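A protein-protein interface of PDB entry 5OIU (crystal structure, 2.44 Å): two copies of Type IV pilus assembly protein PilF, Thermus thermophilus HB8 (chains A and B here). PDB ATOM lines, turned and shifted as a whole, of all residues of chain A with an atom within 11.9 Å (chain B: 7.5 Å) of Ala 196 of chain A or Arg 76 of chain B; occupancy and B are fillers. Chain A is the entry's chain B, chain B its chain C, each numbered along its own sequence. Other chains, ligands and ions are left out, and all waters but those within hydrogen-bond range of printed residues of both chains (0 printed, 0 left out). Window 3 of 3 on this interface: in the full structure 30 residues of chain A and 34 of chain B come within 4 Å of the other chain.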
ATOM      1  N   GLN A 174       7.171   3.191  -2.100  1.00  0.00           N
ATOM      2  CA  GLN A 174       6.387   3.818  -1.041  1.00  0.00           C
ATOM      3  C   GLN A 174       7.227   4.903  -0.397  1.00  0.00           C
ATOM      4  O   GLN A 174       8.418   4.695  -0.147  1.00  0.00           O
ATOM      5  CB  GLN A 174       5.937   2.780  -0.003  1.00  0.00           C
ATOM      6  CG  GLN A 174       5.220   3.318   1.225  1.00  0.00           C
ATOM      7  CD  GLN A 174       3.802   3.743   0.930  1.00  0.00           C
ATOM      8  OE1 GLN A 174       3.003   2.952   0.444  1.00  0.00           O
ATOM      9  NE2 GLN A 174       3.480   5.001   1.218  1.00  0.00           N
ATOM     10  N   THR A 175       6.615   6.065  -0.166  1.00  0.00           N
ATOM     11  CA  THR A 175       7.298   7.230   0.386  1.00  0.00           C
ATOM     12  C   THR A 175       6.601   7.684   1.657  1.00  0.00           C
ATOM     13  O   THR A 175       5.414   7.408   1.878  1.00  0.00           O
ATOM     14  CB  THR A 175       7.329   8.434  -0.583  1.00  0.00           C
ATOM     15  OG1 THR A 175       6.039   9.061  -0.603  1.00  0.00           O
ATOM     16  CG2 THR A 175       7.715   8.025  -1.979  1.00  0.00           C
ATOM     17  N   ILE A 176       7.360   8.386   2.496  1.00  0.00           N
ATOM     18  CA  ILE A 176       6.803   9.151   3.602  1.00  0.00           C
ATOM     19  C   ILE A 176       7.363  10.557   3.473  1.00  0.00           C
ATOM     20  O   ILE A 176       8.578  10.730   3.333  1.00  0.00           O
ATOM     21  CB  ILE A 176       7.107   8.513   4.977  1.00  0.00           C
ATOM     22  CG1 ILE A 176       6.494   9.349   6.102  1.00  0.00           C
ATOM     23  CG2 ILE A 176       8.594   8.229   5.169  1.00  0.00           C
ATOM     24  CD1 ILE A 176       4.977   9.522   5.958  1.00  0.00           C
ATOM     25  N   GLU A 177       6.481  11.552   3.439  1.00  0.00           N
ATOM     26  CA  GLU A 177       6.853  12.899   3.016  1.00  0.00           C
ATOM     27  C   GLU A 177       6.211  13.953   3.919  1.00  0.00           C
ATOM     28  O   GLU A 177       5.163  13.728   4.534  1.00  0.00           O
ATOM     29  CB  GLU A 177       6.445  13.135   1.554  1.00  0.00           C
ATOM     30  CG  GLU A 177       7.241  12.319   0.544  1.00  0.00           C
ATOM     31  CD  GLU A 177       6.873  12.660  -0.890  1.00  0.00           C
ATOM     32  OE1 GLU A 177       7.166  13.795  -1.345  1.00  0.00           O
ATOM     33  OE2 GLU A 177       6.274  11.795  -1.554  1.00  0.00           O
ATOM     34  N   ASP A 178       6.841  15.124   3.983  1.00  0.00           N
ATOM     35  CA  ASP A 178       6.434  16.180   4.915  1.00  0.00           C
ATOM     36  C   ASP A 178       6.599  17.572   4.301  1.00  0.00           C
ATOM     37  O   ASP A 178       7.576  18.283   4.572  1.00  0.00           O
ATOM     38  CB  ASP A 178       7.226  16.066   6.219  1.00  0.00           C
ATOM     39  CG  ASP A 178       6.732  17.034   7.284  1.00  0.00           C
ATOM     40  OD1 ASP A 178       5.524  17.357   7.283  1.00  0.00           O
ATOM     41  OD2 ASP A 178       7.556  17.473   8.115  1.00  0.00           O
ATOM     42  N   GLN A 189       2.248   7.301  -2.029  1.00  0.00           N
ATOM     43  CA  GLN A 189       2.757   8.425  -1.255  1.00  0.00           C
ATOM     44  C   GLN A 189       1.915   8.636  -0.009  1.00  0.00           C
ATOM     45  O   GLN A 189       0.683   8.569  -0.051  1.00  0.00           O
ATOM     46  CB  GLN A 189       2.803   9.689  -2.101  1.00  0.00           C
ATOM     47  CG  GLN A 189       3.735   9.546  -3.296  1.00  0.00           C
ATOM     48  CD  GLN A 189       3.685  10.746  -4.232  1.00  0.00           C
ATOM     49  OE1 GLN A 189       2.965  10.744  -5.231  1.00  0.00           O
ATOM     50  NE2 GLN A 189       4.453  11.779  -3.906  1.00  0.00           N
ATOM     51  N   THR A 190       2.603   8.873   1.104  1.00  0.00           N
ATOM     52  CA  THR A 190       1.994   9.030   2.417  1.00  0.00           C
ATOM     53  C   THR A 190       2.580  10.266   3.074  1.00  0.00           C
ATOM     54  O   THR A 190       3.803  10.445   3.073  1.00  0.00           O
ATOM     55  CB  THR A 190       2.247   7.805   3.295  1.00  0.00           C
ATOM     56  OG1 THR A 190       1.517   6.696   2.759  1.00  0.00           O
ATOM     57  CG2 THR A 190       1.827   8.074   4.757  1.00  0.00           C
ATOM     58  N   GLN A 191       1.706  11.101   3.643  1.00  0.00           N
ATOM     59  CA  GLN A 191       2.087  12.375   4.242  1.00  0.00           C
ATOM     60  C   GLN A 191       2.197  12.253   5.752  1.00  0.00           C
ATOM     61  O   GLN A 191       1.340  11.648   6.402  1.00  0.00           O
ATOM     62  CB  GLN A 191       1.064  13.456   3.894  1.00  0.00           C
ATOM     63  CG  GLN A 191       1.574  14.878   4.063  1.00  0.00           C
ATOM     64  CD  GLN A 191       0.833  15.859   3.178  1.00  0.00           C
ATOM     65  OE1 GLN A 191       1.120  15.988   1.979  1.00  0.00           O
ATOM     66  NE2 GLN A 191      -0.143  16.541   3.753  1.00  0.00           N
ATOM     67  N   VAL A 192       3.260  12.832   6.306  1.00  0.00           N
ATOM     68  CA  VAL A 192       3.350  13.015   7.752  1.00  0.00           C
ATOM     69  C   VAL A 192       2.140  13.821   8.231  1.00  0.00           C
ATOM     70  O   VAL A 192       1.803  14.862   7.654  1.00  0.00           O
ATOM     71  CB  VAL A 192       4.685  13.700   8.098  1.00  0.00           C
ATOM     72  CG1 VAL A 192       4.737  14.139   9.584  1.00  0.00           C
ATOM     73  CG2 VAL A 192       5.853  12.777   7.740  1.00  0.00           C
ATOM     74  N   ASN A 193       1.456  13.328   9.276  1.00  0.00           N
ATOM     75  CA  ASN A 193       0.241  13.966   9.809  1.00  0.00           C
ATOM     76  C   ASN A 193       0.298  14.043  11.335  1.00  0.00           C
ATOM     77  O   ASN A 193      -0.390  13.284  12.034  1.00  0.00           O
ATOM     78  CB  ASN A 193      -1.022  13.225   9.352  1.00  0.00           C
ATOM     79  CG  ASN A 193      -2.312  13.885   9.857  1.00  0.00           C
ATOM     80  OD1 ASN A 193      -2.278  14.978  10.407  1.00  0.00           O
ATOM     81  ND2 ASN A 193      -3.449  13.225   9.654  1.00  0.00           N
ATOM     82  N   PRO A 194       1.074  14.986  11.884  1.00  0.00           N
ATOM     83  CA  PRO A 194       1.294  15.001  13.345  1.00  0.00           C
ATOM     84  C   PRO A 194       0.035  15.241  14.172  1.00  0.00           C
ATOM     85  O   PRO A 194      -0.082  14.679  15.267  1.00  0.00           O
ATOM     86  CB  PRO A 194       2.313  16.138  13.533  1.00  0.00           C
ATOM     87  CG  PRO A 194       2.900  16.382  12.185  1.00  0.00           C
ATOM     88  CD  PRO A 194       1.814  16.063  11.207  1.00  0.00           C
ATOM     89  N   GLN A 195      -0.910  16.056  13.684  1.00  0.00           N
ATOM     90  CA  GLN A 195      -2.206  16.208  14.347  1.00  0.00           C
ATOM     91  C   GLN A 195      -2.859  14.861  14.635  1.00  0.00           C
ATOM     92  O   GLN A 195      -3.733  14.773  15.504  1.00  0.00           O
ATOM     93  CB  GLN A 195      -3.167  17.057  13.489  1.00  0.00           C
ATOM     94  CG  GLN A 195      -2.559  18.289  12.780  1.00  0.00           C
ATOM     95  CD  GLN A 195      -1.951  17.955  11.412  1.00  0.00           C
ATOM     96  OE1 GLN A 195      -0.916  17.283  11.328  1.00  0.00           O
ATOM     97  NE2 GLN A 195      -2.598  18.417  10.337  1.00  0.00           N
ATOM     98  N   ALA A 196      -2.458  13.811  13.921  1.00  0.00           N
ATOM     99  CA  ALA A 196      -3.002  12.480  14.107  1.00  0.00           C
ATOM    100  C   ALA A 196      -1.982  11.494  14.656  1.00  0.00           C
ATOM    101  O   ALA A 196      -2.336  10.347  14.923  1.00  0.00           O
ATOM    102  CB  ALA A 196      -3.573  11.970  12.781  1.00  0.00           C
ATOM    103  N   GLY A 197      -0.734  11.903  14.854  1.00  0.00           N
ATOM    104  CA  GLY A 197       0.278  10.990  15.342  1.00  0.00           C
ATOM    105  C   GLY A 197       1.041  10.228  14.270  1.00  0.00           C
ATOM    106  O   GLY A 197       1.943   9.456  14.609  1.00  0.00           O
ATOM    107  N   LEU A 198       0.725  10.409  12.988  1.00  0.00           N
ATOM    108  CA  LEU A 198       1.471   9.688  11.951  1.00  0.00           C
ATOM    109  C   LEU A 198       2.750  10.462  11.673  1.00  0.00           C
ATOM    110  O   LEU A 198       2.819  11.313  10.778  1.00  0.00           O
ATOM    111  CB  LEU A 198       0.643   9.489  10.683  1.00  0.00           C
ATOM    112  CG  LEU A 198       1.424   8.754   9.588  1.00  0.00           C
ATOM    113  CD1 LEU A 198       1.592   7.281   9.950  1.00  0.00           C
ATOM    114  CD2 LEU A 198       0.745   8.874   8.251  1.00  0.00           C
ATOM    115  N   THR A 199       3.765  10.156  12.469  1.00  0.00           N
ATOM    116  CA  THR A 199       5.088  10.730  12.331  1.00  0.00           C
ATOM    117  C   THR A 199       5.894   9.931  11.317  1.00  0.00           C
ATOM    118  O   THR A 199       5.454   8.889  10.818  1.00  0.00           O
ATOM    119  CB  THR A 199       5.818  10.708  13.663  1.00  0.00           C
ATOM    120  OG1 THR A 199       6.028   9.332  14.007  1.00  0.00           O
ATOM    121  CG2 THR A 199       4.991  11.416  14.778  1.00  0.00           C
ATOM    122  N   PHE A 200       7.119  10.403  11.049  1.00  0.00           N
ATOM    123  CA  PHE A 200       8.020   9.690  10.146  1.00  0.00           C
ATOM    124  C   PHE A 200       8.264   8.257  10.624  1.00  0.00           C
ATOM    125  O   PHE A 200       8.116   7.292   9.858  1.00  0.00           O
ATOM    126  CB  PHE A 200       9.328  10.453  10.028  1.00  0.00           C
ATOM    127  CG  PHE A 200       9.366  11.435   8.885  1.00  0.00           C
ATOM    128  CD1 PHE A 200       9.401  10.984   7.553  1.00  0.00           C
ATOM    129  CD2 PHE A 200       9.398  12.808   9.127  1.00  0.00           C
ATOM    130  CE1 PHE A 200       9.464  11.894   6.484  1.00  0.00           C
ATOM    131  CE2 PHE A 200       9.458  13.727   8.054  1.00  0.00           C
ATOM    132  CZ  PHE A 200       9.491  13.263   6.735  1.00  0.00           C
ATOM    133  N   ALA A 201       8.635   8.102  11.890  1.00  0.00           N
ATOM    134  CA  ALA A 201       8.893   6.772  12.426  1.00  0.00           C
ATOM    135  C   ALA A 201       7.651   5.896  12.375  1.00  0.00           C
ATOM    136  O   ALA A 201       7.740   4.704  12.066  1.00  0.00           O
ATOM    137  CB  ALA A 201       9.411   6.879  13.856  1.00  0.00           C
ATOM    138  N   ARG A 202       6.482   6.460  12.685  1.00  0.00           N
ATOM    139  CA  ARG A 202       5.278   5.636  12.745  1.00  0.00           C
ATOM    140  C   ARG A 202       4.968   5.041  11.376  1.00  0.00           C
ATOM    141  O   ARG A 202       4.698   3.841  11.247  1.00  0.00           O
ATOM    142  CB  ARG A 202       4.112   6.473  13.274  1.00  0.00           C
ATOM    143  CG  ARG A 202       2.762   5.764  13.380  1.00  0.00           C
ATOM    144  CD  ARG A 202       2.647   4.856  14.598  1.00  0.00           C
ATOM    145  NE  ARG A 202       1.325   4.228  14.698  1.00  0.00           N
ATOM    146  CZ  ARG A 202       0.288   4.773  15.330  1.00  0.00           C
ATOM    147  NH1 ARG A 202       0.423   5.960  15.917  1.00  0.00           N
ATOM    148  NH2 ARG A 202      -0.879   4.139  15.372  1.00  0.00           N
ATOM    149  N   ALA A 203       5.031   5.872  10.337  1.00  0.00           N
ATOM    150  CA  ALA A 203       4.854   5.396   8.970  1.00  0.00           C
ATOM    151  C   ALA A 203       5.907   4.361   8.600  1.00  0.00           C
ATOM    152  O   ALA A 203       5.584   3.299   8.049  1.00  0.00           O
ATOM    153  CB  ALA A 203       4.913   6.581   8.006  1.00  0.00           C
ATOM    154  N   LEU A 204       7.177   4.660   8.891  1.00  0.00           N
ATOM    155  CA  LEU A 204       8.259   3.757   8.510  1.00  0.00           C
ATOM    156  C   LEU A 204       8.046   2.362   9.083  1.00  0.00           C
ATOM    157  O   LEU A 204       8.266   1.363   8.389  1.00  0.00           O
ATOM    158  CB  LEU A 204       9.609   4.316   8.959  1.00  0.00           C
ATOM    159  CG  LEU A 204      10.473   5.043   7.933  1.00  0.00           C
ATOM    160  CD1 LEU A 204      11.882   5.219   8.497  1.00  0.00           C
ATOM    161  CD2 LEU A 204      10.487   4.304   6.583  1.00  0.00           C
ATOM    162  N   ALA A 206       5.145   1.078   9.757  1.00  0.00           N
ATOM    163  CA  ALA A 206       4.039   0.516   9.001  1.00  0.00           C
ATOM    164  C   ALA A 206       4.492   0.020   7.630  1.00  0.00           C
ATOM    165  O   ALA A 206       3.990  -1.003   7.144  1.00  0.00           O
ATOM    166  CB  ALA A 206       2.931   1.556   8.866  1.00  0.00           C
ATOM    167  N   PHE A 207       5.443   0.731   6.992  1.00  0.00           N
ATOM    168  CA  PHE A 207       5.907   0.346   5.654  1.00  0.00           C
ATOM    169  C   PHE A 207       6.444  -1.081   5.646  1.00  0.00           C
ATOM    170  O   PHE A 207       6.232  -1.835   4.686  1.00  0.00           O
ATOM    171  CB  PHE A 207       6.995   1.307   5.162  1.00  0.00           C
ATOM    172  CG  PHE A 207       6.508   2.693   4.841  1.00  0.00           C
ATOM    173  CD1 PHE A 207       5.188   3.053   5.035  1.00  0.00           C
ATOM    174  CD2 PHE A 207       7.376   3.627   4.315  1.00  0.00           C
ATOM    175  CE1 PHE A 207       4.750   4.305   4.735  1.00  0.00           C
ATOM    176  CE2 PHE A 207       6.943   4.890   3.986  1.00  0.00           C
ATOM    177  CZ  PHE A 207       5.629   5.241   4.213  1.00  0.00           C
ATOM    178  N   ARG A 209       5.366  -3.621   7.059  1.00  0.00           N
ATOM    179  CA  ARG A 209       4.276  -4.568   6.849  1.00  0.00           C
ATOM    180  C   ARG A 209       3.555  -4.339   5.514  1.00  0.00           C
ATOM    181  O   ARG A 209       2.521  -4.962   5.253  1.00  0.00           O
ATOM    182  CB  ARG A 209       3.297  -4.490   8.029  1.00  0.00           C
ATOM    183  CG  ARG A 209       3.944  -4.069   9.389  1.00  0.00           C
ATOM    184  CD  ARG A 209       2.892  -3.386  10.330  1.00  0.00           C
ATOM    185  NE  ARG A 209       3.390  -2.369  11.293  1.00  0.00           N
ATOM    186  CZ  ARG A 209       2.671  -1.351  11.805  1.00  0.00           C
ATOM    187  NH1 ARG A 209       3.233  -0.510  12.659  1.00  0.00           N
ATOM    188  NH2 ARG A 209       1.392  -1.154  11.469  1.00  0.00           N
ATOM    189  N   GLN A 210       4.076  -3.457   4.664  1.00  0.00           N
ATOM    190  CA  GLN A 210       3.436  -3.116   3.405  1.00  0.00           C
ATOM    191  C   GLN A 210       4.117  -3.773   2.221  1.00  0.00           C
ATOM    192  O   GLN A 210       3.876  -3.372   1.081  1.00  0.00           O
ATOM    193  CB  GLN A 210       3.412  -1.600   3.208  1.00  0.00           C
ATOM    194  CG  GLN A 210       2.323  -0.872   3.977  1.00  0.00           C
ATOM    195  CD  GLN A 210       1.018  -0.827   3.204  1.00  0.00           C
ATOM    196  OE1 GLN A 210       0.988  -0.420   2.039  1.00  0.00           O
ATOM    197  NE2 GLN A 210      -0.064  -1.246   3.844  1.00  0.00           N
ATOM    198  N   LYS B  65     -10.935  -4.618   6.619  1.00  0.00           N
ATOM    199  CA  LYS B  65     -10.710  -4.192   7.998  1.00  0.00           C
ATOM    200  C   LYS B  65     -11.488  -5.060   8.969  1.00  0.00           C
ATOM    201  O   LYS B  65     -10.944  -5.497   9.991  1.00  0.00           O
ATOM    202  CB  LYS B  65     -11.093  -2.723   8.187  1.00  0.00           C
ATOM    203  CG  LYS B  65      -9.941  -1.767   8.065  1.00  0.00           C
ATOM    204  CD  LYS B  65     -10.365  -0.375   8.421  1.00  0.00           C
ATOM    205  CE  LYS B  65      -9.357   0.640   7.941  1.00  0.00           C
ATOM    206  NZ  LYS B  65      -9.606   1.948   8.602  1.00  0.00           N
ATOM    207  N   ALA B  73     -13.423   3.219  11.599  1.00  0.00           N
ATOM    208  CA  ALA B  73     -13.539   4.665  11.751  1.00  0.00           C
ATOM    209  C   ALA B  73     -12.194   5.372  11.635  1.00  0.00           C
ATOM    210  O   ALA B  73     -12.145   6.519  11.176  1.00  0.00           O
ATOM    211  CB  ALA B  73     -14.197   4.995  13.091  1.00  0.00           C
ATOM    212  N   GLU B  74     -11.106   4.707  12.035  1.00  0.00           N
ATOM    213  CA  GLU B  74      -9.762   5.276  11.973  1.00  0.00           C
ATOM    214  C   GLU B  74      -9.193   5.115  10.566  1.00  0.00           C
ATOM    215  O   GLU B  74      -8.926   3.996  10.110  1.00  0.00           O
ATOM    216  CB  GLU B  74      -8.852   4.606  12.999  1.00  0.00           C
ATOM    217  CG  GLU B  74      -7.400   5.024  12.873  1.00  0.00           C
ATOM    218  CD  GLU B  74      -7.201   6.499  13.187  1.00  0.00           C
ATOM    219  OE1 GLU B  74      -7.243   6.851  14.382  1.00  0.00           O
ATOM    220  OE2 GLU B  74      -7.018   7.305  12.248  1.00  0.00           O
ATOM    221  N   LYS B  75      -8.993   6.228   9.874  1.00  0.00           N
ATOM    222  CA  LYS B  75      -8.411   6.193   8.547  1.00  0.00           C
ATOM    223  C   LYS B  75      -7.114   6.980   8.459  1.00  0.00           C
ATOM    224  O   LYS B  75      -6.468   6.967   7.408  1.00  0.00           O
ATOM    225  CB  LYS B  75      -9.417   6.711   7.506  1.00  0.00           C
ATOM    226  CG  LYS B  75     -10.680   5.888   7.428  1.00  0.00           C
ATOM    227  CD  LYS B  75     -11.599   6.372   6.314  1.00  0.00           C
ATOM    228  CE  LYS B  75     -12.638   5.314   5.928  1.00  0.00           C
ATOM    229  NZ  LYS B  75     -13.389   4.775   7.115  1.00  0.00           N
ATOM    230  N   ARG B  76      -6.702   7.644   9.528  1.00  0.00           N
ATOM    231  CA  ARG B  76      -5.529   8.497   9.474  1.00  0.00           C
ATOM    232  C   ARG B  76      -4.277   7.831  10.027  1.00  0.00           C
ATOM    233  O   ARG B  76      -3.174   8.334   9.789  1.00  0.00           O
ATOM    234  CB  ARG B  76      -5.808   9.805  10.216  1.00  0.00           C
ATOM    235  CG  ARG B  76      -6.937  10.616   9.582  1.00  0.00           C
ATOM    236  CD  ARG B  76      -7.202  11.901  10.365  1.00  0.00           C
ATOM    237  NE  ARG B  76      -7.408  11.601  11.778  1.00  0.00           N
ATOM    238  CZ  ARG B  76      -7.107  12.418  12.781  1.00  0.00           C
ATOM    239  NH1 ARG B  76      -6.582  13.618  12.540  1.00  0.00           N
ATOM    240  NH2 ARG B  76      -7.329  12.023  14.031  1.00  0.00           N
ATOM    241  N   LEU B  77      -4.411   6.698  10.713  1.00  0.00           N
ATOM    242  CA  LEU B  77      -3.269   5.962  11.227  1.00  0.00           C
ATOM    243  C   LEU B  77      -3.210   4.567  10.609  1.00  0.00           C
ATOM    244  O   LEU B  77      -4.238   4.033  10.176  1.00  0.00           O
ATOM    245  CB  LEU B  77      -3.346   5.841  12.754  1.00  0.00           C
ATOM    246  CG  LEU B  77      -3.103   7.107  13.578  1.00  0.00           C
ATOM    247  CD1 LEU B  77      -3.337   6.807  15.065  1.00  0.00           C
ATOM    248  CD2 LEU B  77      -1.705   7.682  13.331  1.00  0.00           C
ATOM    249  N   PRO B  78      -2.029   3.948  10.549  1.00  0.00           N
ATOM    250  CA  PRO B  78      -1.943   2.576  10.029  1.00  0.00           C
ATOM    251  C   PRO B  78      -2.219   1.543  11.107  1.00  0.00           C
ATOM    252  O   PRO B  78      -1.814   1.694  12.257  1.00  0.00           O
ATOM    253  CB  PRO B  78      -0.490   2.483   9.540  1.00  0.00           C
ATOM    254  CG  PRO B  78       0.256   3.405  10.438  1.00  0.00           C
ATOM    255  CD  PRO B  78      -0.701   4.522  10.826  1.00  0.00           C
ATOM    256  N   GLN B  79      -2.907   0.465  10.727  1.00  0.00           N
ATOM    257  CA  GLN B  79      -3.268  -0.600  11.657  1.00  0.00           C
ATOM    258  C   GLN B  79      -2.828  -1.951  11.100  1.00  0.00           C
ATOM    259  O   GLN B  79      -2.478  -2.074   9.926  1.00  0.00           O
ATOM    260  CB  GLN B  79      -4.777  -0.576  11.941  1.00  0.00           C
ATOM    261  CG  GLN B  79      -5.359   0.837  11.894  1.00  0.00           C
ATOM    262  CD  GLN B  79      -6.876   0.871  11.777  1.00  0.00           C
ATOM    263  OE1 GLN B  79      -7.583   0.160  12.486  1.00  0.00           O
ATOM    264  NE2 GLN B  79      -7.379   1.712  10.872  1.00  0.00           N
ATOM    265  N   LEU B  99      -2.643   1.314   5.394  1.00  0.00           N
ATOM    266  CA  LEU B  99      -1.787   2.455   5.472  1.00  0.00           C
ATOM    267  C   LEU B  99      -2.459   3.620   4.760  1.00  0.00           C
ATOM    268  O   LEU B  99      -2.860   3.480   3.590  1.00  0.00           O
ATOM    269  CB  LEU B  99      -0.436   2.142   4.839  1.00  0.00           C
ATOM    270  CG  LEU B  99       0.572   3.282   4.715  1.00  0.00           C
ATOM    271  CD1 LEU B  99       1.439   3.354   5.962  1.00  0.00           C
ATOM    272  CD2 LEU B  99       1.432   3.083   3.470  1.00  0.00           C
ATOM    273  N   PRO B 100      -2.600   4.766   5.425  1.00  0.00           N
ATOM    274  CA  PRO B 100      -3.090   5.967   4.735  1.00  0.00           C
ATOM    275  C   PRO B 100      -2.133   6.382   3.626  1.00  0.00           C
ATOM    276  O   PRO B 100      -0.913   6.352   3.797  1.00  0.00           O
ATOM    277  CB  PRO B 100      -3.130   7.034   5.841  1.00  0.00           C
ATOM    278  CG  PRO B 100      -2.757   6.347   7.118  1.00  0.00           C
ATOM    279  CD  PRO B 100      -2.120   5.044   6.791  1.00  0.00           C
ATOM    280  N   THR B 101      -2.699   6.781   2.488  1.00  0.00           N
ATOM    281  CA  THR B 101      -1.952   7.374   1.393  1.00  0.00           C
ATOM    282  C   THR B 101      -2.676   8.621   0.923  1.00  0.00           C
ATOM    283  O   THR B 101      -3.725   9.008   1.452  1.00  0.00           O
ATOM    284  CB  THR B 101      -1.769   6.423   0.200  1.00  0.00           C
ATOM    285  OG1 THR B 101      -3.015   6.297  -0.502  1.00  0.00           O
ATOM    286  CG2 THR B 101      -1.292   5.062   0.662  1.00  0.00           C
ATOM    287  N   GLU B 105      -6.820   4.682   1.695  1.00  0.00           N
ATOM    288  CA  GLU B 105      -6.096   3.655   2.432  1.00  0.00           C
ATOM    289  C   GLU B 105      -5.657   2.526   1.509  1.00  0.00           C
ATOM    290  O   GLU B 105      -6.457   1.990   0.734  1.00  0.00           O
ATOM    291  CB  GLU B 105      -6.946   3.097   3.566  1.00  0.00           C
ATOM    292  CG  GLU B 105      -7.273   4.143   4.603  1.00  0.00           C
ATOM    293  CD  GLU B 105      -8.050   3.562   5.752  1.00  0.00           C
ATOM    294  OE1 GLU B 105      -9.297   3.516   5.650  1.00  0.00           O
ATOM    295  OE2 GLU B 105      -7.405   3.127   6.736  1.00  0.00           O
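No position is printed for both chains. Of the 15 pairs that touch across the chains among the printed residues, none has its exchanged pair printed and touching as well.
Printed residues of chain A that touch a printed residue of chain B: Gln 174, Gln 189, Thr 190, Ala 196, Gly 197, Leu 198, Arg 202, Ala 206, Phe 207 and Gln 210. Hydrophobic or aromatic side chains of chain A that line the printed part of chain B: Ala 196, Leu 198, Ala 206 and Phe 207. Of the 12 printed residues of chain B, 6 touch a printed residue of chain A. Among the printed residues, 15 pairs touch across the chains.
Of the printed residues of chain B, Gln 174 of chain A touches Leu 99 (3.4 Å). Ala 196 of chain A touches just these residues of chain B: Arg 76 (3.4 Å) and Leu 77 (3.2 Å). Of the printed residues of chain B, Leu 198 of chain A touches Leu 77 and Pro 78. Of the printed residues of chain B, Arg 202 of chain A touches Leu 77. No residue of chain A comes within 4 Å of Lys 75 of chain B. Arg 76 of chain B touches just one residue of chain A: Ala 196 (3.4 Å). Leu 77 of chain B touches four residues of chain A. The nearest printed residue of chain A that does not touch Leu 99 of chain B is Ala 203 of chain A (4.6 Å).
OG1 of Thr 190 of chain A sits at hydrogen-bond distance from O of Pro 100 of chain B (2.7 Å).
The backbone NH (N) of Glu 177 of chain A sits at hydrogen-bond distance from the backbone carbonyl oxygen (O) of Thr 190 of chain A (2.9 Å). The side-chain carboxylate (OE2) of Glu 74 of chain B sits at hydrogen-bond distance from the backbone NH (N) of Arg 76 of chain B, at 2.8 Å. The backbone NH of Asn 193 of chain A sits at hydrogen-bond distance from the backbone carbonyl oxygen of Leu 198 of chain A (2.9 Å). The side-chain hydroxyl (OG1) of Thr 199 of chain A sits at hydrogen-bond distance from the backbone NH (N) of Arg 202 of chain A. N of Leu 77 of chain B is in hydrogen-bond range of OE2 of Glu 74 of chain B (3.1 Å). The side-chain amide nitrogen of Gln 174 of chain A lies within hydrogen-bond range of the side-chain hydroxyl of Thr 190 of chain A (3.0 Å).
Among the printed residues, merely in contact across the chains: Gln 174 of chain A with Leu 99 of chain B (3.4 Å), Gln 189 of chain A with Thr 101 of chain B (3.2 Å), Thr 190 of chain A with Leu 99 of chain B (3.7 Å), Thr 190 of chain A with Thr 101 of chain B (3.8 Å), Ala 196 of chain A with Arg 76 of chain B (3.4 Å), Ala 196 of chain A with Leu 77 of chain B (3.2 Å), Gly 197 of chain A with Leu 77 of chain B (3.9 Å), Leu 198 of chain A with Leu 77 of chain B (3.7 Å), Leu 198 of chain A with Pro 78 of chain B (3.7 Å), Arg 202 of chain A with Leu 77 of chain B (3.6 Å), Ala 206 of chain A with Pro 78 of chain B (3.6 Å), Ala 206 of chain A with Leu 99 of chain B (3.7 Å), Phe 207 of chain A with Leu 99 of chain B (3.7 Å) and Gln 210 of chain A with Leu 99 of chain B (3.6 Å).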
